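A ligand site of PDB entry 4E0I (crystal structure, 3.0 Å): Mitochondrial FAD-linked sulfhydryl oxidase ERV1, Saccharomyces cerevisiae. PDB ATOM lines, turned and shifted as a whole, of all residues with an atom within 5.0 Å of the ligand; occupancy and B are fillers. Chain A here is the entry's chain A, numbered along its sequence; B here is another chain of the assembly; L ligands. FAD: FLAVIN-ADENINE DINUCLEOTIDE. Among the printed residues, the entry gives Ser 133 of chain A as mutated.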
ATOM      1  N   VAL A  87     -15.428  -2.445  -2.640  1.00  0.00           N
ATOM      2  CA  VAL A  87     -16.792  -2.622  -3.170  1.00  0.00           C
ATOM      3  C   VAL A  87     -17.371  -4.003  -2.848  1.00  0.00           C
ATOM      4  O   VAL A  87     -18.532  -4.116  -2.453  1.00  0.00           O
ATOM      5  CB  VAL A  87     -16.871  -2.365  -4.695  1.00  0.00           C
ATOM      6  CG1 VAL A  87     -16.684  -0.893  -5.010  1.00  0.00           C
ATOM      7  CG2 VAL A  87     -15.841  -3.203  -5.444  1.00  0.00           C
ATOM      8  N   GLU A  88     -16.547  -5.033  -3.028  1.00  0.00           N
ATOM      9  CA  GLU A  88     -16.940  -6.418  -2.844  1.00  0.00           C
ATOM     10  C   GLU A  88     -17.168  -6.760  -1.366  1.00  0.00           C
ATOM     11  O   GLU A  88     -18.149  -7.428  -1.030  1.00  0.00           O
ATOM     12  CB  GLU A  88     -15.886  -7.362  -3.441  1.00  0.00           C
ATOM     13  CG  GLU A  88     -15.646  -7.195  -4.936  1.00  0.00           C
ATOM     14  CD  GLU A  88     -14.513  -8.054  -5.462  1.00  0.00           C
ATOM     15  OE1 GLU A  88     -14.274  -9.155  -4.908  1.00  0.00           O
ATOM     16  OE2 GLU A  88     -13.863  -7.641  -6.444  1.00  0.00           O
ATOM     17  N   GLY A  91     -20.127  -4.616  -0.090  1.00  0.00           N
ATOM     18  CA  GLY A  91     -21.302  -5.172  -0.740  1.00  0.00           C
ATOM     19  C   GLY A  91     -21.888  -6.384  -0.020  1.00  0.00           C
ATOM     20  O   GLY A  91     -23.063  -6.362   0.357  1.00  0.00           O
ATOM     21  N   ARG A  92     -21.070  -7.410   0.173  1.00  0.00           N
ATOM     22  CA  ARG A  92     -21.520  -8.637   0.834  1.00  0.00           C
ATOM     23  C   ARG A  92     -21.782  -8.455   2.328  1.00  0.00           C
ATOM     24  O   ARG A  92     -22.551  -9.207   2.925  1.00  0.00           O
ATOM     25  CB  ARG A  92     -20.562  -9.806   0.582  1.00  0.00           C
ATOM     26  CG  ARG A  92     -19.246  -9.761   1.355  1.00  0.00           C
ATOM     27  CD  ARG A  92     -18.419 -11.019   1.114  1.00  0.00           C
ATOM     28  NE  ARG A  92     -17.876 -11.066  -0.239  1.00  0.00           N
ATOM     29  CZ  ARG A  92     -16.702 -10.561  -0.605  1.00  0.00           C
ATOM     30  NH1 ARG A  92     -15.922  -9.957   0.294  1.00  0.00           N
ATOM     31  NH2 ARG A  92     -16.293 -10.653  -1.853  1.00  0.00           N
ATOM     32  N   SER A  94     -23.086  -5.620   3.461  1.00  0.00           N
ATOM     33  CA  SER A  94     -24.351  -4.910   3.453  1.00  0.00           C
ATOM     34  C   SER A  94     -25.516  -5.861   3.205  1.00  0.00           C
ATOM     35  O   SER A  94     -26.602  -5.684   3.753  1.00  0.00           O
ATOM     36  CB  SER A  94     -24.343  -3.791   2.399  1.00  0.00           C
ATOM     37  OG  SER A  94     -23.278  -2.889   2.627  1.00  0.00           O
ATOM     38  N   TRP A  95     -25.281  -6.883   2.375  1.00  0.00           N
ATOM     39  CA  TRP A  95     -26.307  -7.880   2.040  1.00  0.00           C
ATOM     40  C   TRP A  95     -26.673  -8.745   3.199  1.00  0.00           C
ATOM     41  O   TRP A  95     -27.860  -9.013   3.420  1.00  0.00           O
ATOM     42  CB  TRP A  95     -25.887  -8.734   0.857  1.00  0.00           C
ATOM     43  CG  TRP A  95     -26.017  -8.037  -0.482  1.00  0.00           C
ATOM     44  CD1 TRP A  95     -25.016  -7.826  -1.424  1.00  0.00           C
ATOM     45  CD2 TRP A  95     -27.227  -7.442  -1.070  1.00  0.00           C
ATOM     46  NE1 TRP A  95     -25.511  -7.161  -2.520  1.00  0.00           N
ATOM     47  CE2 TRP A  95     -26.824  -6.902  -2.376  1.00  0.00           C
ATOM     48  CE3 TRP A  95     -28.550  -7.312  -0.664  1.00  0.00           C
ATOM     49  CZ2 TRP A  95     -27.723  -6.255  -3.215  1.00  0.00           C
ATOM     50  CZ3 TRP A  95     -29.447  -6.655  -1.521  1.00  0.00           C
ATOM     51  CH2 TRP A  95     -29.043  -6.147  -2.763  1.00  0.00           C
ATOM     52  N   LEU A  98     -28.958  -6.689   5.381  1.00  0.00           N
ATOM     53  CA  LEU A  98     -30.238  -6.444   4.710  1.00  0.00           C
ATOM     54  C   LEU A  98     -31.163  -7.664   4.691  1.00  0.00           C
ATOM     55  O   LEU A  98     -32.378  -7.526   4.885  1.00  0.00           O
ATOM     56  CB  LEU A  98     -30.019  -5.929   3.282  1.00  0.00           C
ATOM     57  CG  LEU A  98     -29.606  -4.463   3.113  1.00  0.00           C
ATOM     58  CD1 LEU A  98     -29.002  -4.231   1.742  1.00  0.00           C
ATOM     59  CD2 LEU A  98     -30.776  -3.514   3.348  1.00  0.00           C
ATOM     60  N   HIS A  99     -30.599  -8.843   4.457  1.00  0.00           N
ATOM     61  CA  HIS A  99     -31.379 -10.087   4.469  1.00  0.00           C
ATOM     62  C   HIS A  99     -31.708 -10.537   5.859  1.00  0.00           C
ATOM     63  O   HIS A  99     -32.759 -11.138   6.084  1.00  0.00           O
ATOM     64  CB  HIS A  99     -30.648 -11.192   3.710  1.00  0.00           C
ATOM     65  CG  HIS A  99     -30.554 -10.952   2.223  1.00  0.00           C
ATOM     66  ND1 HIS A  99     -31.630 -10.986   1.411  1.00  0.00           N
ATOM     67  CD2 HIS A  99     -29.463 -10.682   1.409  1.00  0.00           C
ATOM     68  CE1 HIS A  99     -31.250 -10.740   0.155  1.00  0.00           C
ATOM     69  NE2 HIS A  99     -29.923 -10.557   0.149  1.00  0.00           N
ATOM     70  N   PHE A 124     -31.024   4.329   3.063  1.00  0.00           N
ATOM     71  CA  PHE A 124     -29.956   3.433   2.611  1.00  0.00           C
ATOM     72  C   PHE A 124     -29.537   3.730   1.169  1.00  0.00           C
ATOM     73  O   PHE A 124     -28.343   3.845   0.885  1.00  0.00           O
ATOM     74  CB  PHE A 124     -30.392   1.980   2.738  1.00  0.00           C
ATOM     75  CG  PHE A 124     -29.263   0.989   2.648  1.00  0.00           C
ATOM     76  CD1 PHE A 124     -28.513   0.668   3.780  1.00  0.00           C
ATOM     77  CD2 PHE A 124     -28.945   0.378   1.450  1.00  0.00           C
ATOM     78  CE1 PHE A 124     -27.471  -0.233   3.705  1.00  0.00           C
ATOM     79  CE2 PHE A 124     -27.909  -0.533   1.368  1.00  0.00           C
ATOM     80  CZ  PHE A 124     -27.161  -0.841   2.496  1.00  0.00           C
ATOM     81  N   TYR A 128     -25.684   4.999   0.884  1.00  0.00           N
ATOM     82  CA  TYR A 128     -24.831   3.862   0.565  1.00  0.00           C
ATOM     83  C   TYR A 128     -23.509   4.365  -0.036  1.00  0.00           C
ATOM     84  O   TYR A 128     -23.524   5.080  -1.034  1.00  0.00           O
ATOM     85  CB  TYR A 128     -25.513   2.868  -0.381  1.00  0.00           C
ATOM     86  CG  TYR A 128     -24.752   1.572  -0.548  1.00  0.00           C
ATOM     87  CD1 TYR A 128     -24.696   0.632   0.478  1.00  0.00           C
ATOM     88  CD2 TYR A 128     -24.066   1.298  -1.732  1.00  0.00           C
ATOM     89  CE1 TYR A 128     -23.985  -0.552   0.332  1.00  0.00           C
ATOM     90  CE2 TYR A 128     -23.355   0.119  -1.886  1.00  0.00           C
ATOM     91  CZ  TYR A 128     -23.317  -0.798  -0.850  1.00  0.00           C
ATOM     92  OH  TYR A 128     -22.618  -1.970  -1.002  1.00  0.00           O
ATOM     93  N   TRP A 132     -22.235   5.519  -7.239  1.00  0.00           N
ATOM     94  CA  TRP A 132     -22.684   5.005  -8.538  1.00  0.00           C
ATOM     95  C   TRP A 132     -23.545   3.779  -8.435  1.00  0.00           C
ATOM     96  O   TRP A 132     -24.371   3.517  -9.319  1.00  0.00           O
ATOM     97  CB  TRP A 132     -21.484   4.769  -9.464  1.00  0.00           C
ATOM     98  CG  TRP A 132     -20.271   4.156  -8.792  1.00  0.00           C
ATOM     99  CD1 TRP A 132     -19.340   4.799  -7.977  1.00  0.00           C
ATOM    100  CD2 TRP A 132     -19.820   2.759  -8.865  1.00  0.00           C
ATOM    101  NE1 TRP A 132     -18.373   3.918  -7.551  1.00  0.00           N
ATOM    102  CE2 TRP A 132     -18.606   2.685  -8.047  1.00  0.00           C
ATOM    103  CE3 TRP A 132     -20.287   1.608  -9.498  1.00  0.00           C
ATOM    104  CZ2 TRP A 132     -17.902   1.492  -7.885  1.00  0.00           C
ATOM    105  CZ3 TRP A 132     -19.565   0.419  -9.331  1.00  0.00           C
ATOM    106  CH2 TRP A 132     -18.410   0.365  -8.545  1.00  0.00           C
ATOM    107  N   SER A 133     -23.374   3.015  -7.350  1.00  0.00           N
ATOM    108  CA  SER A 133     -24.220   1.846  -7.072  1.00  0.00           C
ATOM    109  C   SER A 133     -25.483   2.243  -6.319  1.00  0.00           C
ATOM    110  O   SER A 133     -26.555   1.675  -6.555  1.00  0.00           O
ATOM    111  CB  SER A 133     -23.444   0.797  -6.272  1.00  0.00           C
ATOM    112  OG  SER A 133     -22.319   0.327  -7.005  1.00  0.00           O
ATOM    113  N   ASP A 136     -28.191   3.635  -8.630  1.00  0.00           N
ATOM    114  CA  ASP A 136     -28.849   2.525  -9.337  1.00  0.00           C
ATOM    115  C   ASP A 136     -29.914   1.866  -8.463  1.00  0.00           C
ATOM    116  O   ASP A 136     -31.032   1.606  -8.936  1.00  0.00           O
ATOM    117  CB  ASP A 136     -27.818   1.470  -9.758  1.00  0.00           C
ATOM    118  CG  ASP A 136     -27.214   1.747 -11.126  1.00  0.00           C
ATOM    119  OD1 ASP A 136     -27.043   2.924 -11.496  1.00  0.00           O
ATOM    120  OD2 ASP A 136     -26.913   0.757 -11.834  1.00  0.00           O
ATOM    121  N   PHE A 137     -29.572   1.606  -7.204  1.00  0.00           N
ATOM    122  CA  PHE A 137     -30.475   0.972  -6.245  1.00  0.00           C
ATOM    123  C   PHE A 137     -31.669   1.860  -5.910  1.00  0.00           C
ATOM    124  O   PHE A 137     -32.771   1.368  -5.700  1.00  0.00           O
ATOM    125  CB  PHE A 137     -29.706   0.586  -4.974  1.00  0.00           C
ATOM    126  CG  PHE A 137     -30.549  -0.149  -3.960  1.00  0.00           C
ATOM    127  CD1 PHE A 137     -31.288  -1.271  -4.314  1.00  0.00           C
ATOM    128  CD2 PHE A 137     -30.577   0.287  -2.635  1.00  0.00           C
ATOM    129  CE1 PHE A 137     -32.051  -1.937  -3.377  1.00  0.00           C
ATOM    130  CE2 PHE A 137     -31.341  -0.385  -1.690  1.00  0.00           C
ATOM    131  CZ  PHE A 137     -32.078  -1.497  -2.061  1.00  0.00           C
ATOM    132  N   MET A 158     -36.426  -8.561  -1.412  1.00  0.00           N
ATOM    133  CA  MET A 158     -34.993  -8.380  -1.183  1.00  0.00           C
ATOM    134  C   MET A 158     -34.161  -9.297  -2.076  1.00  0.00           C
ATOM    135  O   MET A 158     -33.148  -8.876  -2.641  1.00  0.00           O
ATOM    136  CB  MET A 158     -34.648  -8.619   0.286  1.00  0.00           C
ATOM    137  CG  MET A 158     -33.343  -7.987   0.743  1.00  0.00           C
ATOM    138  SD  MET A 158     -33.456  -6.210   1.023  1.00  0.00           S
ATOM    139  CE  MET A 158     -34.418  -6.151   2.544  1.00  0.00           C
ATOM    140  N   CYS A 159     -34.596 -10.551  -2.194  1.00  0.00           N
ATOM    141  CA  CYS A 159     -33.942 -11.549  -3.031  1.00  0.00           C
ATOM    142  C   CYS A 159     -33.948 -11.148  -4.509  1.00  0.00           C
ATOM    143  O   CYS A 159     -32.940 -11.323  -5.207  1.00  0.00           O
ATOM    144  CB  CYS A 159     -34.601 -12.918  -2.853  1.00  0.00           C
ATOM    145  SG  CYS A 159     -33.996 -14.195  -3.984  1.00  0.00           S
ATOM    146  N   HIS A 162     -31.472  -8.231  -4.909  1.00  0.00           N
ATOM    147  CA  HIS A 162     -30.137  -8.816  -4.912  1.00  0.00           C
ATOM    148  C   HIS A 162     -29.867  -9.505  -6.220  1.00  0.00           C
ATOM    149  O   HIS A 162     -28.768  -9.404  -6.770  1.00  0.00           O
ATOM    150  CB  HIS A 162     -30.000  -9.808  -3.753  1.00  0.00           C
ATOM    151  CG  HIS A 162     -28.574 -10.179  -3.400  1.00  0.00           C
ATOM    152  ND1 HIS A 162     -27.579 -10.226  -4.305  1.00  0.00           N
ATOM    153  CD2 HIS A 162     -28.007 -10.554  -2.174  1.00  0.00           C
ATOM    154  CE1 HIS A 162     -26.435 -10.593  -3.700  1.00  0.00           C
ATOM    155  NE2 HIS A 162     -26.698 -10.795  -2.402  1.00  0.00           N
ATOM    156  N   ASN A 163     -30.887 -10.202  -6.742  1.00  0.00           N
ATOM    157  CA  ASN A 163     -30.794 -10.880  -8.034  1.00  0.00           C
ATOM    158  C   ASN A 163     -30.622  -9.948  -9.230  1.00  0.00           C
ATOM    159  O   ASN A 163     -30.065 -10.361 -10.257  1.00  0.00           O
ATOM    160  CB  ASN A 163     -31.994 -11.798  -8.256  1.00  0.00           C
ATOM    161  CG  ASN A 163     -31.787 -13.199  -7.693  1.00  0.00           C
ATOM    162  OD1 ASN A 163     -30.673 -13.575  -7.318  1.00  0.00           O
ATOM    163  ND2 ASN A 163     -32.858 -13.977  -7.643  1.00  0.00           N
ATOM    164  N   VAL A 165     -28.821  -7.111  -9.100  1.00  0.00           N
ATOM    165  CA  VAL A 165     -27.391  -6.810  -9.034  1.00  0.00           C
ATOM    166  C   VAL A 165     -26.587  -8.030  -9.500  1.00  0.00           C
ATOM    167  O   VAL A 165     -25.576  -7.892 -10.182  1.00  0.00           O
ATOM    168  CB  VAL A 165     -26.947  -6.371  -7.617  1.00  0.00           C
ATOM    169  CG1 VAL A 165     -25.450  -6.124  -7.561  1.00  0.00           C
ATOM    170  CG2 VAL A 165     -27.697  -5.112  -7.190  1.00  0.00           C
ATOM    171  N   ASN A 166     -27.070  -9.220  -9.137  1.00  0.00           N
ATOM    172  CA  ASN A 166     -26.466 -10.480  -9.573  1.00  0.00           C
ATOM    173  C   ASN A 166     -26.342 -10.577 -11.097  1.00  0.00           C
ATOM    174  O   ASN A 166     -25.302 -10.980 -11.607  1.00  0.00           O
ATOM    175  CB  ASN A 166     -27.246 -11.687  -9.041  1.00  0.00           C
ATOM    176  CG  ASN A 166     -26.983 -11.949  -7.562  1.00  0.00           C
ATOM    177  OD1 ASN A 166     -25.941 -11.572  -7.022  1.00  0.00           O
ATOM    178  ND2 ASN A 166     -27.940 -12.601  -6.900  1.00  0.00           N
ATOM    179  N   LYS A 168     -26.463  -7.966 -13.197  1.00  0.00           N
ATOM    180  CA  LYS A 168     -25.602  -6.857 -13.599  1.00  0.00           C
ATOM    181  C   LYS A 168     -24.119  -7.200 -13.442  1.00  0.00           C
ATOM    182  O   LYS A 168     -23.273  -6.732 -14.213  1.00  0.00           O
ATOM    183  CB  LYS A 168     -25.939  -5.591 -12.784  1.00  0.00           C
ATOM    184  CG  LYS A 168     -25.318  -4.314 -13.334  1.00  0.00           C
ATOM    185  CD  LYS A 168     -25.331  -3.199 -12.303  1.00  0.00           C
ATOM    186  CE  LYS A 168     -24.338  -2.112 -12.664  1.00  0.00           C
ATOM    187  NZ  LYS A 168     -24.290  -1.034 -11.633  1.00  0.00           N
ATOM    188  N   LEU A 169     -23.807  -8.023 -12.440  1.00  0.00           N
ATOM    189  CA  LEU A 169     -22.436  -8.456 -12.188  1.00  0.00           C
ATOM    190  C   LEU A 169     -22.120  -9.814 -12.815  1.00  0.00           C
ATOM    191  O   LEU A 169     -21.040 -10.366 -12.603  1.00  0.00           O
ATOM    192  CB  LEU A 169     -22.142  -8.459 -10.684  1.00  0.00           C
ATOM    193  CG  LEU A 169     -22.259  -7.112  -9.965  1.00  0.00           C
ATOM    194  CD1 LEU A 169     -21.828  -7.241  -8.513  1.00  0.00           C
ATOM    195  CD2 LEU A 169     -21.443  -6.047 -10.678  1.00  0.00           C
ATOM    196  N   LYS A 171     -23.270 -12.689 -12.106  1.00  0.00           N
ATOM    197  CA  LYS A 171     -23.257 -13.762 -11.127  1.00  0.00           C
ATOM    198  C   LYS A 171     -24.489 -14.631 -11.350  1.00  0.00           C
ATOM    199  O   LYS A 171     -25.457 -14.180 -11.974  1.00  0.00           O
ATOM    200  CB  LYS A 171     -23.257 -13.188  -9.707  1.00  0.00           C
ATOM    201  CG  LYS A 171     -22.154 -12.177  -9.435  1.00  0.00           C
ATOM    202  CD  LYS A 171     -22.029 -11.865  -7.949  1.00  0.00           C
ATOM    203  CE  LYS A 171     -20.925 -10.850  -7.685  1.00  0.00           C
ATOM    204  NZ  LYS A 171     -19.568 -11.377  -8.011  1.00  0.00           N
ATOM    205  N   PHE A 174     -29.763 -16.383  -7.911  1.00  0.00           N
ATOM    206  CA  PHE A 174     -30.106 -17.069  -6.670  1.00  0.00           C
ATOM    207  C   PHE A 174     -31.588 -17.429  -6.613  1.00  0.00           C
ATOM    208  O   PHE A 174     -32.447 -16.612  -6.955  1.00  0.00           O
ATOM    209  CB  PHE A 174     -29.719 -16.188  -5.483  1.00  0.00           C
ATOM    210  CG  PHE A 174     -29.898 -16.835  -4.137  1.00  0.00           C
ATOM    211  CD1 PHE A 174     -31.098 -16.707  -3.436  1.00  0.00           C
ATOM    212  CD2 PHE A 174     -28.856 -17.540  -3.542  1.00  0.00           C
ATOM    213  CE1 PHE A 174     -31.254 -17.297  -2.182  1.00  0.00           C
ATOM    214  CE2 PHE A 174     -29.007 -18.133  -2.301  1.00  0.00           C
ATOM    215  CZ  PHE A 174     -30.204 -18.009  -1.613  1.00  0.00           C
ATOM    216  N   TRP A 179     -34.386 -18.463   0.334  1.00  0.00           N
ATOM    217  CA  TRP A 179     -33.876 -17.308   1.080  1.00  0.00           C
ATOM    218  C   TRP A 179     -34.007 -17.483   2.575  1.00  0.00           C
ATOM    219  O   TRP A 179     -33.137 -17.069   3.332  1.00  0.00           O
ATOM    220  CB  TRP A 179     -34.536 -16.016   0.598  1.00  0.00           C
ATOM    221  CG  TRP A 179     -35.849 -15.698   1.287  1.00  0.00           C
ATOM    222  CD1 TRP A 179     -37.133 -16.032   0.864  1.00  0.00           C
ATOM    223  CD2 TRP A 179     -36.031 -14.966   2.550  1.00  0.00           C
ATOM    224  NE1 TRP A 179     -38.078 -15.571   1.758  1.00  0.00           N
ATOM    225  CE2 TRP A 179     -37.480 -14.921   2.785  1.00  0.00           C
ATOM    226  CE3 TRP A 179     -35.184 -14.361   3.472  1.00  0.00           C
ATOM    227  CZ2 TRP A 179     -38.031 -14.301   3.896  1.00  0.00           C
ATOM    228  CZ3 TRP A 179     -35.745 -13.748   4.589  1.00  0.00           C
ATOM    229  CH2 TRP A 179     -37.131 -13.712   4.793  1.00  0.00           C
ATOM    230  N   ARG A 182     -31.318 -19.832   3.848  1.00  0.00           N
ATOM    231  CA  ARG A 182     -30.018 -19.165   3.825  1.00  0.00           C
ATOM    232  C   ARG A 182     -29.859 -18.132   4.950  1.00  0.00           C
ATOM    233  O   ARG A 182     -28.770 -17.984   5.505  1.00  0.00           O
ATOM    234  CB  ARG A 182     -29.779 -18.519   2.453  1.00  0.00           C
ATOM    235  CG  ARG A 182     -28.546 -17.628   2.339  1.00  0.00           C
ATOM    236  CD  ARG A 182     -27.247 -18.395   2.459  1.00  0.00           C
ATOM    237  NE  ARG A 182     -26.073 -17.526   2.348  1.00  0.00           N
ATOM    238  CZ  ARG A 182     -25.491 -16.889   3.365  1.00  0.00           C
ATOM    239  NH1 ARG A 182     -25.950 -17.033   4.598  1.00  0.00           N
ATOM    240  NH2 ARG A 182     -24.434 -16.123   3.143  1.00  0.00           N
ATOM    241  N   TRP A 183     -30.948 -17.450   5.299  1.00  0.00           N
ATOM    242  CA  TRP A 183     -30.875 -16.255   6.144  1.00  0.00           C
ATOM    243  C   TRP A 183     -31.592 -16.301   7.466  1.00  0.00           C
ATOM    244  O   TRP A 183     -31.261 -15.544   8.377  1.00  0.00           O
ATOM    245  CB  TRP A 183     -31.334 -15.031   5.362  1.00  0.00           C
ATOM    246  CG  TRP A 183     -30.417 -14.676   4.223  1.00  0.00           C
ATOM    247  CD1 TRP A 183     -30.690 -14.752   2.862  1.00  0.00           C
ATOM    248  CD2 TRP A 183     -29.029 -14.215   4.315  1.00  0.00           C
ATOM    249  NE1 TRP A 183     -29.604 -14.355   2.120  1.00  0.00           N
ATOM    250  CE2 TRP A 183     -28.572 -14.016   2.928  1.00  0.00           C
ATOM    251  CE3 TRP A 183     -28.156 -13.927   5.361  1.00  0.00           C
ATOM    252  CZ2 TRP A 183     -27.299 -13.572   2.634  1.00  0.00           C
ATOM    253  CZ3 TRP A 183     -26.868 -13.480   5.048  1.00  0.00           C
ATOM    254  CH2 TRP A 183     -26.454 -13.304   3.722  1.00  0.00           C
ATOM    255  N   TYR B  79     -23.943 -21.286  -5.349  1.00  0.00           N
ATOM    256  CA  TYR B  79     -24.364 -20.937  -3.991  1.00  0.00           C
ATOM    257  C   TYR B  79     -24.454 -22.174  -3.086  1.00  0.00           C
ATOM    258  O   TYR B  79     -25.100 -23.165  -3.421  1.00  0.00           O
ATOM    259  CB  TYR B  79     -25.690 -20.171  -4.011  1.00  0.00           C
ATOM    260  CG  TYR B  79     -25.617 -18.866  -4.786  1.00  0.00           C
ATOM    261  CD1 TYR B  79     -24.841 -17.797  -4.329  1.00  0.00           C
ATOM    262  CD2 TYR B  79     -26.329 -18.706  -5.970  1.00  0.00           C
ATOM    263  CE1 TYR B  79     -24.785 -16.606  -5.033  1.00  0.00           C
ATOM    264  CE2 TYR B  79     -26.268 -17.519  -6.687  1.00  0.00           C
ATOM    265  CZ  TYR B  79     -25.491 -16.468  -6.217  1.00  0.00           C
ATOM    266  OH  TYR B  79     -25.433 -15.290  -6.917  1.00  0.00           O
HETATM  267  PA  FAD L   1     -22.806 -11.336  -2.661  1.00  0.00           P
HETATM  268  O1A FAD L   1     -22.927 -10.013  -1.945  1.00  0.00           O
HETATM  269  O2A FAD L   1     -23.162 -11.200  -4.121  1.00  0.00           O
HETATM  270  O5B FAD L   1     -23.753 -12.412  -1.927  1.00  0.00           O
HETATM  271  C5B FAD L   1     -23.495 -12.765  -0.594  1.00  0.00           C
HETATM  272  C4B FAD L   1     -24.241 -14.036  -0.210  1.00  0.00           C
HETATM  273  O4B FAD L   1     -25.639 -13.818  -0.228  1.00  0.00           O
HETATM  274  C3B FAD L   1     -23.958 -15.198  -1.147  1.00  0.00           C
HETATM  275  O3B FAD L   1     -22.944 -16.032  -0.619  1.00  0.00           O
HETATM  276  C2B FAD L   1     -25.292 -15.921  -1.266  1.00  0.00           C
HETATM  277  O2B FAD L   1     -25.335 -17.046  -0.430  1.00  0.00           O
HETATM  278  C1B FAD L   1     -26.327 -14.899  -0.807  1.00  0.00           C
HETATM  279  N9A FAD L   1     -27.143 -14.410  -1.945  1.00  0.00           N
HETATM  280  C8A FAD L   1     -26.718 -14.144  -3.230  1.00  0.00           C
HETATM  281  N7A FAD L   1     -27.762 -13.704  -3.953  1.00  0.00           N
HETATM  282  C5A FAD L   1     -28.850 -13.662  -3.169  1.00  0.00           C
HETATM  283  C6A FAD L   1     -30.179 -13.294  -3.405  1.00  0.00           C
HETATM  284  N6A FAD L   1     -30.571 -12.981  -4.641  1.00  0.00           N
HETATM  285  N1A FAD L   1     -31.099 -13.355  -2.377  1.00  0.00           N
HETATM  286  C2A FAD L   1     -30.714 -13.793  -1.132  1.00  0.00           C
HETATM  287  N3A FAD L   1     -29.394 -14.164  -0.898  1.00  0.00           N
HETATM  288  C4A FAD L   1     -28.483 -14.096  -1.901  1.00  0.00           C
HETATM  289  N1  FAD L   1     -21.502  -4.069  -6.791  1.00  0.00           N
HETATM  290  C2  FAD L   1     -21.257  -3.684  -8.091  1.00  0.00           C
HETATM  291  O2  FAD L   1     -20.222  -4.050  -8.651  1.00  0.00           O
HETATM  292  N3  FAD L   1     -22.165  -2.893  -8.780  1.00  0.00           N
HETATM  293  C4  FAD L   1     -23.333  -2.492  -8.150  1.00  0.00           C
HETATM  294  O4  FAD L   1     -24.137  -1.789  -8.758  1.00  0.00           O
HETATM  295  C4X FAD L   1     -23.591  -2.876  -6.839  1.00  0.00           C
HETATM  296  N5  FAD L   1     -24.749  -2.473  -6.207  1.00  0.00           N
HETATM  297  C5X FAD L   1     -25.006  -2.852  -4.905  1.00  0.00           C
HETATM  298  C6  FAD L   1     -26.191  -2.432  -4.301  1.00  0.00           C
HETATM  299  C7  FAD L   1     -26.465  -2.802  -2.984  1.00  0.00           C
HETATM  300  C7M FAD L   1     -27.750  -2.330  -2.366  1.00  0.00           C
HETATM  301  C8  FAD L   1     -25.556  -3.610  -2.283  1.00  0.00           C
HETATM  302  C8M FAD L   1     -25.825  -4.030  -0.866  1.00  0.00           C
HETATM  303  C9  FAD L   1     -24.379  -4.028  -2.898  1.00  0.00           C
HETATM  304  C9A FAD L   1     -24.096  -3.656  -4.212  1.00  0.00           C
HETATM  305  N10 FAD L   1     -22.914  -4.077  -4.839  1.00  0.00           N
HETATM  306  C10 FAD L   1     -22.670  -3.673  -6.152  1.00  0.00           C
HETATM  307  C1' FAD L   1     -22.078  -5.171  -4.230  1.00  0.00           C
HETATM  308  C2' FAD L   1     -22.414  -6.550  -4.812  1.00  0.00           C
HETATM  309  O2' FAD L   1     -23.813  -6.730  -4.815  1.00  0.00           O
HETATM  310  C3' FAD L   1     -21.800  -7.731  -4.052  1.00  0.00           C
HETATM  311  O3' FAD L   1     -22.197  -7.679  -2.698  1.00  0.00           O
HETATM  312  C4' FAD L   1     -20.270  -7.851  -4.133  1.00  0.00           C
HETATM  313  O4' FAD L   1     -19.856  -7.840  -5.483  1.00  0.00           O
HETATM  314  C5' FAD L   1     -19.775  -9.139  -3.475  1.00  0.00           C
HETATM  315  O5' FAD L   1     -20.314 -10.265  -4.138  1.00  0.00           O
HETATM  316  P   FAD L   1     -20.156 -11.756  -3.552  1.00  0.00           P
HETATM  317  O1P FAD L   1     -20.380 -12.762  -4.659  1.00  0.00           O
HETATM  318  O2P FAD L   1     -18.801 -11.971  -2.911  1.00  0.00           O
HETATM  319  O3P FAD L   1     -21.318 -11.921  -2.444  1.00  0.00           O
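N6A of the ligand is in hydrogen-bond range of OD1 of Asn 163, at 2.7 Å. O2' of the ligand lies within hydrogen-bond range of NE1 of Trp 95 (2.9 Å). The guanidinium group of Arg 182 sits at hydrogen-bond distance from an oxygen (O2B) of the ligand, at 2.9 Å. The backbone carbonyl oxygen (O) of Cys 159 is in hydrogen-bond range of a nitrogen (N6A) of the ligand (2.9 Å). SG of Cys 159 sits at hydrogen-bond distance from N6A of the ligand (3.7 Å). N of Arg 92 is in hydrogen-bond range of O3' of the ligand (3.1 Å). NE of Arg 92 is in salt-bridge range of O2P of the ligand. An oxygen (O4) of the ligand lies within hydrogen-bond range of the side-chain amino group (NZ) of Lys 168, at 3.0 Å. O of Gly 91 lies close to O3' of the ligand, at 3.4 Å. N3A of the ligand lies within hydrogen-bond range of NE1 of Trp 183 (3.0 Å). ND2 of Asn 166 is in hydrogen-bond range of N7A of the ligand (3.2 Å). The side-chain hydroxyl (OG) of Ser 133 lies close to an oxygen (O4) of the ligand, at 3.3 Å. A ring nitrogen (NE2) of His 162 is in hydrogen-bond range of an oxygen (O5B) of the ligand (3.4 Å). The side-chain amino group of Lys 171 lies within salt-bridge range of an oxygen (O1P) of the ligand, at 3.7 Å.
The side-chain amide oxygen of Asn 163 lies within hydrogen-bond range of the side-chain amide nitrogen of Asn 166 (2.9 Å). The backbone carbonyl oxygen of Phe 174 lies within hydrogen-bond range of the side-chain amide nitrogen of Asn 163, 2.8 Å away. The guanidinium group (NH2) of Arg 92 is in salt-bridge range of the side-chain carboxylate (OE1) of Glu 88 (3.96 Å). The side-chain carboxylate (OD2) of Asp 136 is in salt-bridge range of the side-chain amino group (NZ) of Lys 168 (3.2 Å). ND2 of Asn 166 lies close to O of His 162 (3.3 Å). The backbone carbonyl oxygen (O) of Asn 166 sits at hydrogen-bond distance from the backbone NH (N) of Lys 171 (2.7 Å).
Glu 88 touches the ligand (O to C5', 3.4 Å). Ser 94 touches the ligand (CB to C8M, 3.6 Å). CE1 of His 99 touches C2A of the ligand, at 3.4 Å. Tyr 128 touches the ligand. CD2 of Phe 137 touches C7M of the ligand (3.9 Å). Val 165 touches the ligand. Leu 169 touches the ligand (CD2 to O2, 3.1 Å). Phe 174 touches the ligand (CB to N6A, 3.4 Å). Tyr 79 of chain B touches the ligand. Hydrophobic or aromatic side chains that line the ligand: Trp 95, His 99, Tyr 128, Phe 137, His 162, Val 165, Leu 169, Phe 174, Trp 183 and Tyr 79 of chain B. 21 residues have an atom within 4 Å of the ligand: Glu 88, Gly 91, Arg 92, Ser 94, Trp 95, His 99, Tyr 128, Ser 133, Phe 137, Cys 159, His 162, Asn 163, Val 165, Asn 166, Lys 168, Leu 169, Lys 171, Phe 174, Arg 182, Trp 183 and Tyr 79 of chain B.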
